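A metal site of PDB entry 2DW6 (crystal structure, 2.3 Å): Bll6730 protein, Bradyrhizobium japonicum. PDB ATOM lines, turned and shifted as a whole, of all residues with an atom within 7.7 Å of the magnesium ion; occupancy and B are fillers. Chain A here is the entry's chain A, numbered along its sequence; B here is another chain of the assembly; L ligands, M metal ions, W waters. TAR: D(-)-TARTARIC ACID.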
ATOM      1  N   ASN A  21     -31.331 -21.626  22.300  1.00  0.00           N
ATOM      2  CA  ASN A  21     -30.662 -21.393  21.032  1.00  0.00           C
ATOM      3  C   ASN A  21     -31.160 -20.035  20.532  1.00  0.00           C
ATOM      4  O   ASN A  21     -31.915 -19.365  21.239  1.00  0.00           O
ATOM      5  CB  ASN A  21     -30.922 -22.524  20.016  1.00  0.00           C
ATOM      6  CG  ASN A  21     -32.388 -22.701  19.667  1.00  0.00           C
ATOM      7  OD1 ASN A  21     -33.113 -21.719  19.471  1.00  0.00           O
ATOM      8  ND2 ASN A  21     -32.819 -23.948  19.552  1.00  0.00           N
ATOM      9  N   ASN A  55     -36.621 -33.754  19.671  1.00  0.00           N
ATOM     10  CA  ASN A  55     -36.706 -32.535  20.464  1.00  0.00           C
ATOM     11  C   ASN A  55     -37.130 -31.359  19.595  1.00  0.00           C
ATOM     12  O   ASN A  55     -36.904 -31.360  18.377  1.00  0.00           O
ATOM     13  CB  ASN A  55     -35.329 -32.190  21.027  1.00  0.00           C
ATOM     14  CG  ASN A  55     -34.323 -31.901  19.918  1.00  0.00           C
ATOM     15  OD1 ASN A  55     -33.758 -32.817  19.316  1.00  0.00           O
ATOM     16  ND2 ASN A  55     -34.119 -30.619  19.625  1.00  0.00           N
ATOM     17  N   TYR A 151     -22.301 -37.089  14.612  1.00  0.00           N
ATOM     18  CA  TYR A 151     -21.620 -35.916  15.130  1.00  0.00           C
ATOM     19  C   TYR A 151     -22.343 -35.497  16.410  1.00  0.00           C
ATOM     20  O   TYR A 151     -23.532 -35.784  16.566  1.00  0.00           O
ATOM     21  CB  TYR A 151     -21.629 -34.782  14.107  1.00  0.00           C
ATOM     22  CG  TYR A 151     -22.986 -34.128  13.864  1.00  0.00           C
ATOM     23  CD1 TYR A 151     -23.371 -32.997  14.593  1.00  0.00           C
ATOM     24  CD2 TYR A 151     -23.861 -34.628  12.899  1.00  0.00           C
ATOM     25  CE1 TYR A 151     -24.602 -32.376  14.363  1.00  0.00           C
ATOM     26  CE2 TYR A 151     -25.093 -34.015  12.663  1.00  0.00           C
ATOM     27  CZ  TYR A 151     -25.458 -32.885  13.405  1.00  0.00           C
ATOM     28  OH  TYR A 151     -26.671 -32.275  13.169  1.00  0.00           O
ATOM     29  N   ALA A 153     -24.012 -32.786  18.830  1.00  0.00           N
ATOM     30  CA  ALA A 153     -24.648 -31.475  18.803  1.00  0.00           C
ATOM     31  C   ALA A 153     -24.897 -30.966  20.218  1.00  0.00           C
ATOM     32  O   ALA A 153     -25.392 -31.691  21.076  1.00  0.00           O
ATOM     33  CB  ALA A 153     -25.975 -31.554  18.046  1.00  0.00           C
ATOM     34  N   TYR A 156     -25.176 -25.034  23.425  1.00  0.00           N
ATOM     35  CA  TYR A 156     -26.322 -24.137  23.603  1.00  0.00           C
ATOM     36  C   TYR A 156     -25.964 -23.025  24.589  1.00  0.00           C
ATOM     37  O   TYR A 156     -24.970 -23.119  25.314  1.00  0.00           O
ATOM     38  CB  TYR A 156     -27.511 -24.910  24.181  1.00  0.00           C
ATOM     39  CG  TYR A 156     -28.225 -25.786  23.177  1.00  0.00           C
ATOM     40  CD1 TYR A 156     -29.316 -25.294  22.450  1.00  0.00           C
ATOM     41  CD2 TYR A 156     -27.817 -27.095  22.951  1.00  0.00           C
ATOM     42  CE1 TYR A 156     -29.965 -26.087  21.507  1.00  0.00           C
ATOM     43  CE2 TYR A 156     -28.457 -27.903  22.022  1.00  0.00           C
ATOM     44  CZ  TYR A 156     -29.535 -27.391  21.300  1.00  0.00           C
ATOM     45  OH  TYR A 156     -30.164 -28.192  20.378  1.00  0.00           O
ATOM     46  N   LYS A 182     -21.223 -29.569  16.971  1.00  0.00           N
ATOM     47  CA  LYS A 182     -22.051 -28.446  16.530  1.00  0.00           C
ATOM     48  C   LYS A 182     -22.441 -27.593  17.729  1.00  0.00           C
ATOM     49  O   LYS A 182     -22.673 -28.103  18.824  1.00  0.00           O
ATOM     50  CB  LYS A 182     -23.308 -28.958  15.808  1.00  0.00           C
ATOM     51  CG  LYS A 182     -24.115 -27.857  15.134  1.00  0.00           C
ATOM     52  CD  LYS A 182     -25.198 -28.403  14.224  1.00  0.00           C
ATOM     53  CE  LYS A 182     -26.369 -28.969  15.007  1.00  0.00           C
ATOM     54  NZ  LYS A 182     -27.413 -29.523  14.082  1.00  0.00           N
ATOM     55  N   VAL A 212     -21.834 -24.795  13.019  1.00  0.00           N
ATOM     56  CA  VAL A 212     -22.605 -23.790  13.734  1.00  0.00           C
ATOM     57  C   VAL A 212     -24.067 -23.801  13.259  1.00  0.00           C
ATOM     58  O   VAL A 212     -24.363 -24.079  12.084  1.00  0.00           O
ATOM     59  CB  VAL A 212     -22.002 -22.375  13.539  1.00  0.00           C
ATOM     60  CG1 VAL A 212     -20.593 -22.337  14.119  1.00  0.00           C
ATOM     61  CG2 VAL A 212     -21.982 -21.994  12.075  1.00  0.00           C
ATOM     62  N   ASP A 213     -24.979 -23.493  14.174  1.00  0.00           N
ATOM     63  CA  ASP A 213     -26.409 -23.517  13.885  1.00  0.00           C
ATOM     64  C   ASP A 213     -27.066 -22.210  14.314  1.00  0.00           C
ATOM     65  O   ASP A 213     -27.018 -21.834  15.490  1.00  0.00           O
ATOM     66  CB  ASP A 213     -27.041 -24.691  14.653  1.00  0.00           C
ATOM     67  CG  ASP A 213     -28.426 -25.032  14.168  1.00  0.00           C
ATOM     68  OD1 ASP A 213     -29.114 -24.146  13.618  1.00  0.00           O
ATOM     69  OD2 ASP A 213     -28.827 -26.206  14.372  1.00  0.00           O
ATOM     70  N   ALA A 214     -27.683 -21.517  13.362  1.00  0.00           N
ATOM     71  CA  ALA A 214     -28.359 -20.244  13.646  1.00  0.00           C
ATOM     72  C   ALA A 214     -29.857 -20.452  13.934  1.00  0.00           C
ATOM     73  O   ALA A 214     -30.564 -19.499  14.282  1.00  0.00           O
ATOM     74  CB  ALA A 214     -28.165 -19.275  12.476  1.00  0.00           C
ATOM     75  N   ASN A 215     -30.316 -21.679  13.769  1.00  0.00           N
ATOM     76  CA  ASN A 215     -31.705 -22.023  14.025  1.00  0.00           C
ATOM     77  C   ASN A 215     -32.766 -21.166  13.322  1.00  0.00           C
ATOM     78  O   ASN A 215     -33.825 -20.903  13.877  1.00  0.00           O
ATOM     79  CB  ASN A 215     -31.942 -22.010  15.534  1.00  0.00           C
ATOM     80  CG  ASN A 215     -31.436 -23.278  16.210  1.00  0.00           C
ATOM     81  OD1 ASN A 215     -32.068 -24.333  16.112  1.00  0.00           O
ATOM     82  ND2 ASN A 215     -30.291 -23.182  16.858  1.00  0.00           N
ATOM     83  N   GLY A 216     -32.452 -20.756  12.092  1.00  0.00           N
ATOM     84  CA  GLY A 216     -33.375 -19.969  11.284  1.00  0.00           C
ATOM     85  C   GLY A 216     -33.767 -18.607  11.811  1.00  0.00           C
ATOM     86  O   GLY A 216     -34.801 -18.059  11.417  1.00  0.00           O
ATOM     87  N   TRP A 237     -19.964 -26.825   8.739  1.00  0.00           N
ATOM     88  CA  TRP A 237     -21.143 -26.321   8.050  1.00  0.00           C
ATOM     89  C   TRP A 237     -21.832 -25.194   8.820  1.00  0.00           C
ATOM     90  O   TRP A 237     -21.636 -25.027  10.011  1.00  0.00           O
ATOM     91  CB  TRP A 237     -22.136 -27.444   7.717  1.00  0.00           C
ATOM     92  CG  TRP A 237     -23.005 -27.948   8.851  1.00  0.00           C
ATOM     93  CD1 TRP A 237     -23.722 -27.197   9.754  1.00  0.00           C
ATOM     94  CD2 TRP A 237     -23.313 -29.308   9.135  1.00  0.00           C
ATOM     95  NE1 TRP A 237     -24.456 -28.011  10.567  1.00  0.00           N
ATOM     96  CE2 TRP A 237     -24.222 -29.312  10.225  1.00  0.00           C
ATOM     97  CE3 TRP A 237     -22.909 -30.531   8.579  1.00  0.00           C
ATOM     98  CZ2 TRP A 237     -24.739 -30.493  10.769  1.00  0.00           C
ATOM     99  CZ3 TRP A 237     -23.426 -31.712   9.123  1.00  0.00           C
ATOM    100  CH2 TRP A 237     -24.329 -31.683  10.202  1.00  0.00           C
ATOM    101  N   GLU A 239     -25.530 -23.987   9.545  1.00  0.00           N
ATOM    102  CA  GLU A 239     -26.903 -24.502   9.526  1.00  0.00           C
ATOM    103  C   GLU A 239     -28.068 -23.542   9.713  1.00  0.00           C
ATOM    104  O   GLU A 239     -27.998 -22.613  10.523  1.00  0.00           O
ATOM    105  CB  GLU A 239     -27.022 -25.619  10.574  1.00  0.00           C
ATOM    106  CG  GLU A 239     -28.384 -26.323  10.624  1.00  0.00           C
ATOM    107  CD  GLU A 239     -28.393 -27.495  11.602  1.00  0.00           C
ATOM    108  OE1 GLU A 239     -27.369 -28.189  11.712  1.00  0.00           O
ATOM    109  OE2 GLU A 239     -29.440 -27.728  12.252  1.00  0.00           O
ATOM    110  N   GLU A 240     -29.143 -23.811   8.973  1.00  0.00           N
ATOM    111  CA  GLU A 240     -30.396 -23.050   9.007  1.00  0.00           C
ATOM    112  C   GLU A 240     -30.194 -21.557   9.304  1.00  0.00           C
ATOM    113  O   GLU A 240     -30.545 -21.063  10.376  1.00  0.00           O
ATOM    114  CB  GLU A 240     -31.351 -23.695  10.031  1.00  0.00           C
ATOM    115  CG  GLU A 240     -32.802 -23.202   9.959  1.00  0.00           C
ATOM    116  CD  GLU A 240     -33.759 -24.024  10.817  1.00  0.00           C
ATOM    117  OE1 GLU A 240     -33.500 -24.220  12.022  1.00  0.00           O
ATOM    118  OE2 GLU A 240     -34.798 -24.472  10.272  1.00  0.00           O
ATOM    119  N   ALA A 262     -26.286 -26.138   5.653  1.00  0.00           N
ATOM    120  CA  ALA A 262     -27.262 -27.176   5.916  1.00  0.00           C
ATOM    121  C   ALA A 262     -28.588 -26.613   6.386  1.00  0.00           C
ATOM    122  O   ALA A 262     -28.639 -25.528   6.985  1.00  0.00           O
ATOM    123  CB  ALA A 262     -26.711 -28.157   6.965  1.00  0.00           C
ATOM    124  N   THR A 263     -29.668 -27.346   6.122  1.00  0.00           N
ATOM    125  CA  THR A 263     -30.989 -26.933   6.551  1.00  0.00           C
ATOM    126  C   THR A 263     -31.963 -28.075   6.333  1.00  0.00           C
ATOM    127  O   THR A 263     -31.581 -29.136   5.840  1.00  0.00           O
ATOM    128  CB  THR A 263     -31.473 -25.702   5.772  1.00  0.00           C
ATOM    129  OG1 THR A 263     -32.651 -25.182   6.390  1.00  0.00           O
ATOM    130  CG2 THR A 263     -31.779 -26.067   4.321  1.00  0.00           C
ATOM    131  N   GLU A 265     -34.324 -29.408   8.902  1.00  0.00           N
ATOM    132  CA  GLU A 265     -34.934 -30.013  10.086  1.00  0.00           C
ATOM    133  C   GLU A 265     -36.370 -29.531  10.314  1.00  0.00           C
ATOM    134  O   GLU A 265     -37.189 -30.269  10.844  1.00  0.00           O
ATOM    135  CB  GLU A 265     -34.097 -29.721  11.332  1.00  0.00           C
ATOM    136  CG  GLU A 265     -34.249 -28.316  11.880  1.00  0.00           C
ATOM    137  CD  GLU A 265     -33.273 -28.023  13.012  1.00  0.00           C
ATOM    138  OE1 GLU A 265     -32.049 -28.132  12.776  1.00  0.00           O
ATOM    139  OE2 GLU A 265     -33.730 -27.687  14.127  1.00  0.00           O
ATOM    140  N   ASN A 266     -36.673 -28.302   9.911  1.00  0.00           N
ATOM    141  CA  ASN A 266     -38.007 -27.748  10.091  1.00  0.00           C
ATOM    142  C   ASN A 266     -38.925 -27.801   8.874  1.00  0.00           C
ATOM    143  O   ASN A 266     -39.874 -27.018   8.765  1.00  0.00           O
ATOM    144  CB  ASN A 266     -37.912 -26.319  10.634  1.00  0.00           C
ATOM    145  CG  ASN A 266     -37.376 -26.275  12.060  1.00  0.00           C
ATOM    146  OD1 ASN A 266     -37.849 -26.994  12.937  1.00  0.00           O
ATOM    147  ND2 ASN A 266     -36.371 -25.439  12.294  1.00  0.00           N
ATOM    148  N   GLN A 290     -31.239 -31.921   6.241  1.00  0.00           N
ATOM    149  CA  GLN A 290     -31.496 -32.489   7.556  1.00  0.00           C
ATOM    150  C   GLN A 290     -32.911 -32.888   7.932  1.00  0.00           C
ATOM    151  O   GLN A 290     -33.291 -32.832   9.102  1.00  0.00           O
ATOM    152  CB  GLN A 290     -30.928 -31.521   8.591  1.00  0.00           C
ATOM    153  CG  GLN A 290     -29.478 -31.171   8.283  1.00  0.00           C
ATOM    154  CD  GLN A 290     -28.952 -29.987   9.062  1.00  0.00           C
ATOM    155  OE1 GLN A 290     -29.513 -28.899   9.019  1.00  0.00           O
ATOM    156  NE2 GLN A 290     -27.854 -30.192   9.787  1.00  0.00           N
ATOM    157  N   HIS A 322     -31.868 -34.724  11.393  1.00  0.00           N
ATOM    158  CA  HIS A 322     -31.853 -34.002  12.647  1.00  0.00           C
ATOM    159  C   HIS A 322     -32.553 -34.944  13.643  1.00  0.00           C
ATOM    160  O   HIS A 322     -33.205 -35.894  13.228  1.00  0.00           O
ATOM    161  CB  HIS A 322     -32.656 -32.700  12.492  1.00  0.00           C
ATOM    162  CG  HIS A 322     -33.262 -32.186  13.757  1.00  0.00           C
ATOM    163  ND1 HIS A 322     -34.335 -32.815  14.372  1.00  0.00           N
ATOM    164  CD2 HIS A 322     -32.922 -31.151  14.552  1.00  0.00           C
ATOM    165  CE1 HIS A 322     -34.620 -32.176  15.490  1.00  0.00           C
ATOM    166  NE2 HIS A 322     -33.782 -31.165  15.627  1.00  0.00           N
ATOM    167  N   GLU A 341     -27.352 -37.184  13.401  1.00  0.00           N
ATOM    168  CA  GLU A 341     -27.032 -36.251  14.471  1.00  0.00           C
ATOM    169  C   GLU A 341     -27.088 -37.017  15.792  1.00  0.00           C
ATOM    170  O   GLU A 341     -27.725 -38.064  15.878  1.00  0.00           O
ATOM    171  CB  GLU A 341     -28.039 -35.104  14.504  1.00  0.00           C
ATOM    172  CG  GLU A 341     -27.732 -34.058  15.534  1.00  0.00           C
ATOM    173  CD  GLU A 341     -28.671 -32.861  15.474  1.00  0.00           C
ATOM    174  OE1 GLU A 341     -28.325 -31.826  16.076  1.00  0.00           O
ATOM    175  OE2 GLU A 341     -29.749 -32.974  14.831  1.00  0.00           O
ATOM    176  N   TYR A 343     -27.049 -36.293  20.318  1.00  0.00           N
ATOM    177  CA  TYR A 343     -27.014 -35.378  21.458  1.00  0.00           C
ATOM    178  C   TYR A 343     -26.503 -36.192  22.648  1.00  0.00           C
ATOM    179  O   TYR A 343     -27.290 -36.766  23.402  1.00  0.00           O
ATOM    180  CB  TYR A 343     -28.410 -34.848  21.792  1.00  0.00           C
ATOM    181  CG  TYR A 343     -29.150 -34.200  20.651  1.00  0.00           C
ATOM    182  CD1 TYR A 343     -28.827 -32.917  20.218  1.00  0.00           C
ATOM    183  CD2 TYR A 343     -30.206 -34.863  20.023  1.00  0.00           C
ATOM    184  CE1 TYR A 343     -29.529 -32.299  19.184  1.00  0.00           C
ATOM    185  CE2 TYR A 343     -30.922 -34.265  18.985  1.00  0.00           C
ATOM    186  CZ  TYR A 343     -30.578 -32.982  18.580  1.00  0.00           C
ATOM    187  OH  TYR A 343     -31.292 -32.381  17.570  1.00  0.00           O
ATOM    188  N   LYS B 102     -40.738 -23.188  17.518  1.00  0.00           N
ATOM    189  CA  LYS B 102     -39.726 -23.173  16.473  1.00  0.00           C
ATOM    190  C   LYS B 102     -40.340 -22.843  15.118  1.00  0.00           C
ATOM    191  O   LYS B 102     -41.524 -23.103  14.887  1.00  0.00           O
ATOM    192  CB  LYS B 102     -38.998 -24.531  16.409  1.00  0.00           C
ATOM    193  CG  LYS B 102     -38.025 -24.755  17.554  1.00  0.00           C
ATOM    194  CD  LYS B 102     -37.274 -26.091  17.459  1.00  0.00           C
ATOM    195  CE  LYS B 102     -36.402 -26.164  16.200  1.00  0.00           C
ATOM    196  NZ  LYS B 102     -35.575 -27.413  16.157  1.00  0.00           N
HETATM  197  O1  TAR L   1     -30.068 -30.053  16.642  1.00  0.00           O
HETATM  198  O11 TAR L   1     -30.405 -29.237  14.627  1.00  0.00           O
HETATM  199  C1  TAR L   1     -30.478 -29.119  15.955  1.00  0.00           C
HETATM  200  C2  TAR L   1     -31.062 -27.892  16.610  1.00  0.00           C
HETATM  201  O2  TAR L   1     -31.628 -26.958  15.702  1.00  0.00           O
HETATM  202  C3  TAR L   1     -32.162 -28.310  17.595  1.00  0.00           C
HETATM  203  O3  TAR L   1     -33.283 -28.930  16.930  1.00  0.00           O
HETATM  204  C4  TAR L   1     -32.592 -27.085  18.380  1.00  0.00           C
HETATM  205  O4  TAR L   1     -31.787 -26.615  19.173  1.00  0.00           O
HETATM  206  O41 TAR L   1     -33.803 -26.535  18.199  1.00  0.00           O
HETATM  207 MG    MG M   1     -30.499 -27.250  13.951  1.00  0.00          MG
HETATM  208  O   HOH W   1     -31.254 -25.636  13.178  1.00  0.00           O
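OD2 of Asp 213 sits close to NZ of Lys 182 (3.6 Å). The backbone NH (N) of Asn 215 is in hydrogen-bond range of the side-chain carboxylate (OD1) of Asp 213, 2.7 Å away. The side-chain amide nitrogen of Gln 290 lies within hydrogen-bond range of the side-chain carboxylate of Glu 239 (2.8 Å). The side-chain carboxylate (OE1) of Glu 239 sits at hydrogen-bond distance from the indole nitrogen (NE1) of Trp 237 (3.1 Å). The backbone NH (N) of Glu 239 is in hydrogen-bond range of the backbone carbonyl oxygen (O) of Val 212. The side-chain carboxylate of Glu 265 is in salt-bridge range of the side-chain amino group of Lys 102 of chain B (2.8 Å). The side-chain carboxylate (OE1) of Glu 341 lies within salt-bridge range of the side-chain amino group (NZ) of Lys 182 (3.2 Å). The backbone carbonyl oxygen of Glu 240 lies within hydrogen-bond range of the backbone NH of Asn 215, 3.5 Å away.
Lys 182 touches the magnesium ion (NZ to MG, 3.8 Å). Asn 215 touches the magnesium ion. The nearest printed residue that does not touch the magnesium ion is His 322 (4.6 Å).
Water W1 is bound to the magnesium ion (1.9 Å). The magnesium ion is bound by the side-chain carboxylate (OD2) of Asp 213 (2.0 Å). The magnesium ion is bound by the side-chain carboxylate (OE2) of Glu 239 (2.1 Å). The magnesium ion is bound by an oxygen (O11) of the ligand (2.1 Å). The magnesium ion is bound by O2 of the ligand. The magnesium ion is bound by OE1 of Glu 265, 2.1 Å away. The magnesium ion has six donor atoms within binding distance.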
